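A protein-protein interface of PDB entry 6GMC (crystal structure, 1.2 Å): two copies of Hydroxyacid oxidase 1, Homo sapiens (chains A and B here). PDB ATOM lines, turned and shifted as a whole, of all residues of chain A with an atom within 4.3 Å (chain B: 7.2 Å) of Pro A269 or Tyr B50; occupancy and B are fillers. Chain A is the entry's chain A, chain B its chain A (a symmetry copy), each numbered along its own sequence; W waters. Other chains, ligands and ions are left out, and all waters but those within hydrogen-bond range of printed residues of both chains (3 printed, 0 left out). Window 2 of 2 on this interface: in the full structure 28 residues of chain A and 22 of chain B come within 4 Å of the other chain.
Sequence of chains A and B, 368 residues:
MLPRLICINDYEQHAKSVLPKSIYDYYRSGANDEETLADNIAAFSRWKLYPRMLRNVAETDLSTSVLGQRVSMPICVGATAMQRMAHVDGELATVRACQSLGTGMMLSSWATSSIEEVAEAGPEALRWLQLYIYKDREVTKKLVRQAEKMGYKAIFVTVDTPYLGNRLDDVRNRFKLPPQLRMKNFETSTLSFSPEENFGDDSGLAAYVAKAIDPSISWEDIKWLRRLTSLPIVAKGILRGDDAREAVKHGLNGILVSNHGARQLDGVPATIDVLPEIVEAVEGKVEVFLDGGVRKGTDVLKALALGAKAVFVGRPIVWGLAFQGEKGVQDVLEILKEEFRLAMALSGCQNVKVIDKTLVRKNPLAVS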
ATOM      1  N   THR A  36      -6.509  22.554  -7.205  1.00  0.00           N
ATOM      2  CA  THR A  36      -5.068  22.820  -7.296  1.00  0.00           C
ATOM      3  C   THR A  36      -4.692  23.246  -8.726  1.00  0.00           C
ATOM      4  O   THR A  36      -3.800  24.069  -8.911  1.00  0.00           O
ATOM      5  CB  THR A  36      -4.266  21.608  -6.809  1.00  0.00           C
ATOM      6  OG1 THR A  36      -4.627  21.332  -5.451  1.00  0.00           O
ATOM      7  CG2 THR A  36      -2.775  21.807  -6.933  1.00  0.00           C
ATOM      8  N   ARG A 240       6.427  19.107   1.193  1.00  0.00           N
ATOM      9  CA  ARG A 240       6.651  19.415   2.604  1.00  0.00           C
ATOM     10  C   ARG A 240       8.142  19.596   2.878  1.00  0.00           C
ATOM     11  O   ARG A 240       8.969  18.830   2.374  1.00  0.00           O
ATOM     12  CB  ARG A 240       6.176  18.271   3.499  1.00  0.00           C
ATOM     13  CG  ARG A 240       4.679  18.017   3.502  1.00  0.00           C
ATOM     14  CD  ARG A 240       4.351  16.757   4.276  1.00  0.00           C
ATOM     15  NE  ARG A 240       4.693  16.840   5.683  1.00  0.00           N
ATOM     16  CZ  ARG A 240       3.831  17.009   6.679  1.00  0.00           C
ATOM     17  NH1 ARG A 240       4.306  17.080   7.908  1.00  0.00           N
ATOM     18  NH2 ARG A 240       2.525  17.092   6.479  1.00  0.00           N
ATOM     19  N   ASN A 259       3.318  19.234  -7.681  1.00  0.00           N
ATOM     20  CA  ASN A 259       2.075  18.552  -7.339  1.00  0.00           C
ATOM     21  C   ASN A 259       1.582  17.746  -8.546  1.00  0.00           C
ATOM     22  O   ASN A 259       0.393  17.452  -8.665  1.00  0.00           O
ATOM     23  CB  ASN A 259       1.035  19.516  -6.765  1.00  0.00           C
ATOM     24  CG  ASN A 259       0.782  20.733  -7.625  1.00  0.00           C
ATOM     25  OD1 ASN A 259       0.844  20.644  -8.859  1.00  0.00           O
ATOM     26  ND2 ASN A 259       0.490  21.865  -6.982  1.00  0.00           N
ATOM     27  N   GLY A 267      -6.300  19.743  -3.840  1.00  0.00           N
ATOM     28  CA  GLY A 267      -6.374  20.522  -2.618  1.00  0.00           C
ATOM     29  C   GLY A 267      -5.035  20.698  -1.934  1.00  0.00           C
ATOM     30  O   GLY A 267      -4.990  21.273  -0.854  1.00  0.00           O
ATOM     31  N   VAL A 268      -3.950  20.226  -2.555  1.00  0.00           N
ATOM     32  CA  VAL A 268      -2.625  20.621  -2.119  1.00  0.00           C
ATOM     33  C   VAL A 268      -2.368  22.049  -2.578  1.00  0.00           C
ATOM     34  O   VAL A 268      -3.016  22.546  -3.503  1.00  0.00           O
ATOM     35  CB  VAL A 268      -1.562  19.634  -2.627  1.00  0.00           C
ATOM     36  CG1 VAL A 268      -1.863  18.214  -2.188  1.00  0.00           C
ATOM     37  CG2 VAL A 268      -1.392  19.688  -4.137  1.00  0.00           C
ATOM     38  N   PRO A 269      -1.407  22.756  -1.959  1.00  0.00           N
ATOM     39  CA  PRO A 269      -1.103  24.115  -2.391  1.00  0.00           C
ATOM     40  C   PRO A 269      -0.476  24.156  -3.789  1.00  0.00           C
ATOM     41  O   PRO A 269       0.027  23.140  -4.303  1.00  0.00           O
ATOM     42  CB  PRO A 269      -0.089  24.628  -1.361  1.00  0.00           C
ATOM     43  CG  PRO A 269      -0.204  23.671  -0.205  1.00  0.00           C
ATOM     44  CD  PRO A 269      -0.574  22.338  -0.821  1.00  0.00           C
ATOM     45  N   ALA A 270      -0.504  25.354  -4.368  1.00  0.00           N
ATOM     46  CA  ALA A 270       0.256  25.640  -5.559  1.00  0.00           C
ATOM     47  C   ALA A 270       1.749  25.453  -5.279  1.00  0.00           C
ATOM     48  O   ALA A 270       2.253  25.762  -4.184  1.00  0.00           O
ATOM     49  CB  ALA A 270       0.003  27.059  -5.986  1.00  0.00           C
ATOM     50  N   THR A 271       2.490  24.992  -6.284  1.00  0.00           N
ATOM     51  CA  THR A 271       3.914  24.787  -6.104  1.00  0.00           C
ATOM     52  C   THR A 271       4.649  26.094  -5.798  1.00  0.00           C
ATOM     53  O   THR A 271       5.574  26.098  -5.002  1.00  0.00           O
ATOM     54  CB  THR A 271       4.507  24.046  -7.299  1.00  0.00           C
ATOM     55  OG1 THR A 271       4.108  24.755  -8.470  1.00  0.00           O
ATOM     56  CG2 THR A 271       4.065  22.594  -7.333  1.00  0.00           C
ATOM     57  N   VAL A 274       4.487  26.708  -2.025  1.00  0.00           N
ATOM     58  CA  VAL A 274       5.267  25.874  -1.096  1.00  0.00           C
ATOM     59  C   VAL A 274       6.771  25.995  -1.372  1.00  0.00           C
ATOM     60  O   VAL A 274       7.584  25.636  -0.526  1.00  0.00           O
ATOM     61  CB  VAL A 274       4.822  24.404  -1.062  1.00  0.00           C
ATOM     62  CG1 VAL A 274       3.419  24.240  -0.515  1.00  0.00           C
ATOM     63  CG2 VAL A 274       4.943  23.715  -2.385  1.00  0.00           C
ATOM     64  N   GLU A 277       9.148  27.390   1.443  1.00  0.00           N
ATOM     65  CA  GLU A 277       9.283  26.474   2.572  1.00  0.00           C
ATOM     66  C   GLU A 277      10.374  25.440   2.263  1.00  0.00           C
ATOM     67  O   GLU A 277      11.201  25.096   3.103  1.00  0.00           O
ATOM     68  CB  GLU A 277       7.923  25.811   2.857  1.00  0.00           C
ATOM     69  CG  GLU A 277       6.930  26.762   3.509  1.00  0.00           C
ATOM     70  CD  GLU A 277       5.422  26.487   3.500  1.00  0.00           C
ATOM     71  OE1 GLU A 277       4.871  25.796   2.590  1.00  0.00           O
ATOM     72  OE2 GLU A 277       4.768  27.020   4.413  1.00  0.00           O
ATOM     73  N   TRP B  47      -8.993  24.838   3.133  1.00  0.00           N
ATOM     74  CA  TRP B  47      -8.068  24.011   3.901  1.00  0.00           C
ATOM     75  C   TRP B  47      -7.222  23.199   2.923  1.00  0.00           C
ATOM     76  O   TRP B  47      -7.754  22.395   2.182  1.00  0.00           O
ATOM     77  CB  TRP B  47      -8.835  23.104   4.861  1.00  0.00           C
ATOM     78  CG  TRP B  47      -9.395  23.812   6.053  1.00  0.00           C
ATOM     79  CD1 TRP B  47     -10.660  24.293   6.218  1.00  0.00           C
ATOM     80  CD2 TRP B  47      -8.686  24.131   7.260  1.00  0.00           C
ATOM     81  NE1 TRP B  47     -10.798  24.863   7.457  1.00  0.00           N
ATOM     82  CE2 TRP B  47      -9.596  24.791   8.109  1.00  0.00           C
ATOM     83  CE3 TRP B  47      -7.380  23.909   7.707  1.00  0.00           C
ATOM     84  CZ2 TRP B  47      -9.236  25.223   9.382  1.00  0.00           C
ATOM     85  CZ3 TRP B  47      -7.020  24.348   8.957  1.00  0.00           C
ATOM     86  CH2 TRP B  47      -7.939  24.990   9.785  1.00  0.00           C
ATOM     87  N   LYS B  48      -5.916  23.447   2.903  1.00  0.00           N
ATOM     88  CA  LYS B  48      -5.029  22.801   1.951  1.00  0.00           C
ATOM     89  C   LYS B  48      -4.324  21.616   2.607  1.00  0.00           C
ATOM     90  O   LYS B  48      -4.051  21.622   3.808  1.00  0.00           O
ATOM     91  CB  LYS B  48      -4.035  23.823   1.399  1.00  0.00           C
ATOM     92  CG  LYS B  48      -4.683  24.975   0.637  1.00  0.00           C
ATOM     93  CD  LYS B  48      -5.405  24.529  -0.626  1.00  0.00           C
ATOM     94  CE  LYS B  48      -6.138  25.639  -1.353  1.00  0.00           C
ATOM     95  NZ  LYS B  48      -6.681  25.161  -2.651  1.00  0.00           N
ATOM     96  N   LEU B  49      -4.030  20.612   1.777  1.00  0.00           N
ATOM     97  CA  LEU B  49      -3.407  19.373   2.207  1.00  0.00           C
ATOM     98  C   LEU B  49      -1.902  19.403   1.938  1.00  0.00           C
ATOM     99  O   LEU B  49      -1.445  19.832   0.879  1.00  0.00           O
ATOM    100  CB  LEU B  49      -4.054  18.203   1.467  1.00  0.00           C
ATOM    101  CG  LEU B  49      -5.453  17.844   1.958  1.00  0.00           C
ATOM    102  CD1 LEU B  49      -6.188  17.015   0.925  1.00  0.00           C
ATOM    103  CD2 LEU B  49      -5.382  17.090   3.274  1.00  0.00           C
ATOM    104  N   TYR B  50      -1.163  18.847   2.899  1.00  0.00           N
ATOM    105  CA  TYR B  50       0.289  18.780   2.891  1.00  0.00           C
ATOM    106  C   TYR B  50       0.696  17.319   2.967  1.00  0.00           C
ATOM    107  O   TYR B  50       1.020  16.803   4.039  1.00  0.00           O
ATOM    108  CB  TYR B  50       0.864  19.624   4.028  1.00  0.00           C
ATOM    109  CG  TYR B  50       0.696  21.097   3.776  1.00  0.00           C
ATOM    110  CD1 TYR B  50      -0.534  21.710   3.931  1.00  0.00           C
ATOM    111  CD2 TYR B  50       1.748  21.862   3.297  1.00  0.00           C
ATOM    112  CE1 TYR B  50      -0.713  23.046   3.620  1.00  0.00           C
ATOM    113  CE2 TYR B  50       1.590  23.207   3.005  1.00  0.00           C
ATOM    114  CZ  TYR B  50       0.350  23.798   3.158  1.00  0.00           C
ATOM    115  OH  TYR B  50       0.169  25.127   2.897  1.00  0.00           O
ATOM    116  N   PRO B  51       0.637  16.599   1.832  1.00  0.00           N
ATOM    117  CA  PRO B  51       0.829  15.155   1.839  1.00  0.00           C
ATOM    118  C   PRO B  51       2.277  14.751   2.114  1.00  0.00           C
ATOM    119  O   PRO B  51       3.212  15.404   1.669  1.00  0.00           O
ATOM    120  CB  PRO B  51       0.457  14.742   0.412  1.00  0.00           C
ATOM    121  CG  PRO B  51       0.757  15.964  -0.411  1.00  0.00           C
ATOM    122  CD  PRO B  51       0.340  17.109   0.489  1.00  0.00           C
ATOM    123  N   ARG B  52       2.431  13.653   2.861  1.00  0.00           N
ATOM    124  CA  ARG B  52       3.727  13.029   3.072  1.00  0.00           C
ATOM    125  C   ARG B  52       3.948  11.968   1.999  1.00  0.00           C
ATOM    126  O   ARG B  52       3.052  11.158   1.717  1.00  0.00           O
ATOM    127  CB  ARG B  52       3.817  12.339   4.431  1.00  0.00           C
ATOM    128  CG  ARG B  52       3.815  13.293   5.610  1.00  0.00           C
ATOM    129  CD  ARG B  52       4.024  12.487   6.875  1.00  0.00           C
ATOM    130  NE  ARG B  52       4.014  13.292   8.077  1.00  0.00           N
ATOM    131  CZ  ARG B  52       2.927  13.606   8.771  1.00  0.00           C
ATOM    132  NH1 ARG B  52       3.056  14.273   9.904  1.00  0.00           N
ATOM    133  NH2 ARG B  52       1.725  13.271   8.328  1.00  0.00           N
ATOM    134  N   MET B  53       5.162  11.968   1.441  1.00  0.00           N
ATOM    135  CA  MET B  53       5.564  11.021   0.426  1.00  0.00           C
ATOM    136  C   MET B  53       6.299   9.826   1.053  1.00  0.00           C
ATOM    137  O   MET B  53       6.870   9.909   2.148  1.00  0.00           O
ATOM    138  CB  MET B  53       6.473  11.708  -0.600  1.00  0.00           C
ATOM    139  CG  MET B  53       5.840  12.943  -1.212  1.00  0.00           C
ATOM    140  SD  MET B  53       4.302  12.557  -2.056  1.00  0.00           S
ATOM    141  CE  MET B  53       3.453  14.128  -1.925  1.00  0.00           C
ATOM    142  N   LEU B 346      -2.656   8.956  -1.097  1.00  0.00           N
ATOM    143  CA  LEU B 346      -1.834   9.981  -1.728  1.00  0.00           C
ATOM    144  C   LEU B 346      -1.235  10.938  -0.692  1.00  0.00           C
ATOM    145  O   LEU B 346      -0.262  11.622  -1.001  1.00  0.00           O
ATOM    146  CB  LEU B 346      -2.652  10.749  -2.762  1.00  0.00           C
ATOM    147  CG  LEU B 346      -3.126   9.943  -3.964  1.00  0.00           C
ATOM    148  CD1 LEU B 346      -3.862  10.863  -4.923  1.00  0.00           C
ATOM    149  CD2 LEU B 346      -1.978   9.216  -4.659  1.00  0.00           C
ATOM    150  N   SER B 347      -1.795  10.980   0.520  1.00  0.00           N
ATOM    151  CA  SER B 347      -1.265  11.859   1.571  1.00  0.00           C
ATOM    152  C   SER B 347      -0.337  11.111   2.534  1.00  0.00           C
ATOM    153  O   SER B 347       0.177  11.727   3.464  1.00  0.00           O
ATOM    154  CB  SER B 347      -2.376  12.555   2.315  1.00  0.00           C
ATOM    155  OG  SER B 347      -3.166  11.635   3.058  1.00  0.00           O
ATOM    156  N   ASP B 356      -3.024  13.344  10.981  1.00  0.00           N
ATOM    157  CA  ASP B 356      -2.620  14.335  11.974  1.00  0.00           C
ATOM    158  C   ASP B 356      -2.904  15.760  11.470  1.00  0.00           C
ATOM    159  O   ASP B 356      -3.130  16.004  10.299  1.00  0.00           O
ATOM    160  CB  ASP B 356      -1.133  14.222  12.341  1.00  0.00           C
ATOM    161  CG  ASP B 356      -0.196  14.521  11.178  1.00  0.00           C
ATOM    162  OD1 ASP B 356      -0.321  13.835  10.127  1.00  0.00           O
ATOM    163  OD2 ASP B 356       0.634  15.460  11.314  1.00  0.00           O
ATOM    164  N   LYS B 357      -2.825  16.720  12.391  1.00  0.00           N
ATOM    165  CA  LYS B 357      -3.099  18.134  12.105  1.00  0.00           C
ATOM    166  C   LYS B 357      -2.050  18.724  11.151  1.00  0.00           C
ATOM    167  O   LYS B 357      -2.336  19.717  10.506  1.00  0.00           O
ATOM    168  CB  LYS B 357      -3.127  18.966  13.392  1.00  0.00           C
ATOM    169  CG  LYS B 357      -1.837  18.963  14.201  1.00  0.00           C
ATOM    170  CD  LYS B 357      -1.954  19.674  15.533  1.00  0.00           C
ATOM    171  CE  LYS B 357      -0.648  19.694  16.298  1.00  0.00           C
ATOM    172  NZ  LYS B 357      -0.786  20.375  17.608  1.00  0.00           N
ATOM    173  N   THR B 358      -0.851  18.125  11.029  1.00  0.00           N
ATOM    174  CA  THR B 358       0.142  18.708  10.084  1.00  0.00           C
ATOM    175  C   THR B 358      -0.236  18.437   8.627  1.00  0.00           C
ATOM    176  O   THR B 358       0.360  19.023   7.713  1.00  0.00           O
ATOM    177  CB  THR B 358       1.595  18.239  10.244  1.00  0.00           C
ATOM    178  OG1 THR B 358       1.765  16.954   9.642  1.00  0.00           O
ATOM    179  CG2 THR B 358       2.053  18.253  11.684  1.00  0.00           C
ATOM    180  N   LEU B 359      -1.245  17.597   8.398  1.00  0.00           N
ATOM    181  CA  LEU B 359      -1.702  17.355   7.037  1.00  0.00           C
ATOM    182  C   LEU B 359      -2.452  18.553   6.447  1.00  0.00           C
ATOM    183  O   LEU B 359      -2.646  18.563   5.235  1.00  0.00           O
ATOM    184  CB  LEU B 359      -2.593  16.117   7.010  1.00  0.00           C
ATOM    185  CG  LEU B 359      -1.865  14.779   7.075  1.00  0.00           C
ATOM    186  CD1 LEU B 359      -2.873  13.656   7.234  1.00  0.00           C
ATOM    187  CD2 LEU B 359      -0.997  14.547   5.839  1.00  0.00           C
ATOM    188  N   VAL B 360      -2.924  19.502   7.268  1.00  0.00           N
ATOM    189  CA  VAL B 360      -3.722  20.615   6.753  1.00  0.00           C
ATOM    190  C   VAL B 360      -3.210  21.966   7.251  1.00  0.00           C
ATOM    191  O   VAL B 360      -2.642  22.102   8.338  1.00  0.00           O
ATOM    192  CB  VAL B 360      -5.214  20.452   7.085  1.00  0.00           C
ATOM    193  CG1 VAL B 360      -5.800  19.242   6.384  1.00  0.00           C
ATOM    194  CG2 VAL B 360      -5.473  20.408   8.579  1.00  0.00           C
ATOM    195  N   ARG B 361      -3.462  22.983   6.424  1.00  0.00           N
ATOM    196  CA  ARG B 361      -3.220  24.376   6.796  1.00  0.00           C
ATOM    197  C   ARG B 361      -4.253  25.229   6.061  1.00  0.00           C
ATOM    198  O   ARG B 361      -4.512  24.966   4.894  1.00  0.00           O
ATOM    199  CB  ARG B 361      -1.794  24.784   6.392  1.00  0.00           C
ATOM    200  CG  ARG B 361      -1.252  26.078   6.978  1.00  0.00           C
ATOM    201  CD  ARG B 361       0.062  26.451   6.296  1.00  0.00           C
ATOM    202  NE  ARG B 361       1.134  25.452   6.409  1.00  0.00           N
ATOM    203  CZ  ARG B 361       2.302  25.512   5.755  1.00  0.00           C
ATOM    204  NH1 ARG B 361       2.534  26.492   4.899  1.00  0.00           N
ATOM    205  NH2 ARG B 361       3.228  24.585   5.933  1.00  0.00           N
ATOM    206  N   LYS B 362      -4.806  26.253   6.715  1.00  0.00           N
ATOM    207  CA  LYS B 362      -5.830  27.072   6.033  1.00  0.00           C
ATOM    208  C   LYS B 362      -5.156  28.203   5.253  1.00  0.00           C
ATOM    209  O   LYS B 362      -4.244  28.849   5.755  1.00  0.00           O
ATOM    210  CB  LYS B 362      -6.884  27.637   6.990  1.00  0.00           C
ATOM    211  CG  LYS B 362      -8.088  28.252   6.277  1.00  0.00           C
ATOM    212  CD  LYS B 362      -8.952  29.134   7.141  1.00  0.00           C
ATOM    213  CE  LYS B 362      -9.725  28.364   8.188  1.00  0.00           C
ATOM    214  NZ  LYS B 362     -10.540  29.262   9.042  1.00  0.00           N
HETATM  215  O   HOH W   1       2.222  26.647   1.583  1.00  0.00           O
HETATM  216  O   HOH W   2       5.788  16.084   0.613  1.00  0.00           O
HETATM  217  O   HOH W   3      -4.423  24.764  -4.205  1.00  0.00           O
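The guanidinium group of Arg A240 lies within hydrogen-bond range of the backbone carbonyl oxygen of Tyr B50 (2.9 Å). NH1 of Arg A240 lies within hydrogen-bond range of OG1 of Thr B358. The backbone carbonyl oxygen (O) of Gly A267 sits at hydrogen-bond distance from the backbone NH (N) of Leu B49, 2.9 Å away. The side-chain carboxylate of Glu A277 is in salt-bridge range of the guanidinium group of Arg B361.
The side-chain hydroxyl of Thr A36 lies within hydrogen-bond range of the backbone NH of Gly A267. ND2 of Asn A259 lies within hydrogen-bond range of O of Pro A269, 3.0 Å away. The backbone NH (N) of Lys B48 is in hydrogen-bond range of the backbone carbonyl oxygen (O) of Arg B361, 2.9 Å away. N of Tyr B50 is in hydrogen-bond range of O of Leu B359 (2.8 Å). OD1 of Asp B356 is in salt-bridge range of NH2 of Arg B52. The guanidinium group (NH1) of Arg B52 is in hydrogen-bond range of the side-chain hydroxyl (OG1) of Thr B358, at 3.0 Å.
Among the printed residues, pairs that only touch across the chains: Arg A240 with Pro B51 (3.2 Å), Pro A269 with Leu B49 (3.2 Å), Gly A267 with Lys B48 (3.2 Å), Val A268 with Leu B49 (3.3 Å), Pro A269 with Tyr B50 (3.4 Å), Val A268 with Pro B51 (3.6 Å) and Arg A240 with Arg B52 (3.7 Å).
Of chain B, only Leu B49 and Tyr B50 come within 4 Å of Pro A269. Ala A270 touches none of the printed residues of chain B. Printed residues of chain B within 4 Å of Glu A277: Arg B361. Of the printed residues of chain A, Lys B48 touches Gly A267. Of the printed residues of chain A, Tyr B50 touches Arg A240 (2.9 Å) and Pro A269 (3.4 Å). Printed residues of chain A within 4 Å of Pro B51: Arg A240 (3.2 Å) and Val A268 (3.6 Å). Of the printed residues of chain A, Thr B358 touches Arg A240 (3.1 Å). The nearest residue of chain B that does not touch Pro A269 is Lys B48 (4.2 Å).
Of the 10 printed residues of chain A, 5 touch a printed residue of chain B. Hydrophobic or aromatic side chains of chain A within 4 Å of the printed part of chain B: Val A268 and Pro A269. Of the 16 printed residues of chain B, 7 touch a printed residue of chain A. Hydrophobic or aromatic side chains of chain B that line the printed part of chain A: Leu B49, Tyr B50 and Pro B51. Among the printed residues, 11 pairs touch across the chains. Among the printed residues, Asp or Glu carboxylates within 4 Å of a Lys or Arg side-chain nitrogen of the other chain: Glu A277 with Arg B361.
No position is printed for both chains. Of the 11 pairs that touch across the chains among the printed residues, none has its exchanged pair printed and touching as well.
Water W3 lies within hydrogen-bond range of the backbone carbonyl oxygen (O) of Val A268 and the side-chain amino group (NZ) of Lys B48. Water W2 bridges O of Pro B51 (2.9 Å) and N of Arg A240 (3.1 Å). Water W1 lies within hydrogen-bond range of the side-chain hydroxyl of Tyr B50 (2.9 Å), the side-chain carboxylate of Glu A277 (3.0 Å) and the guanidinium group of Arg B361 (3.3 Å).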
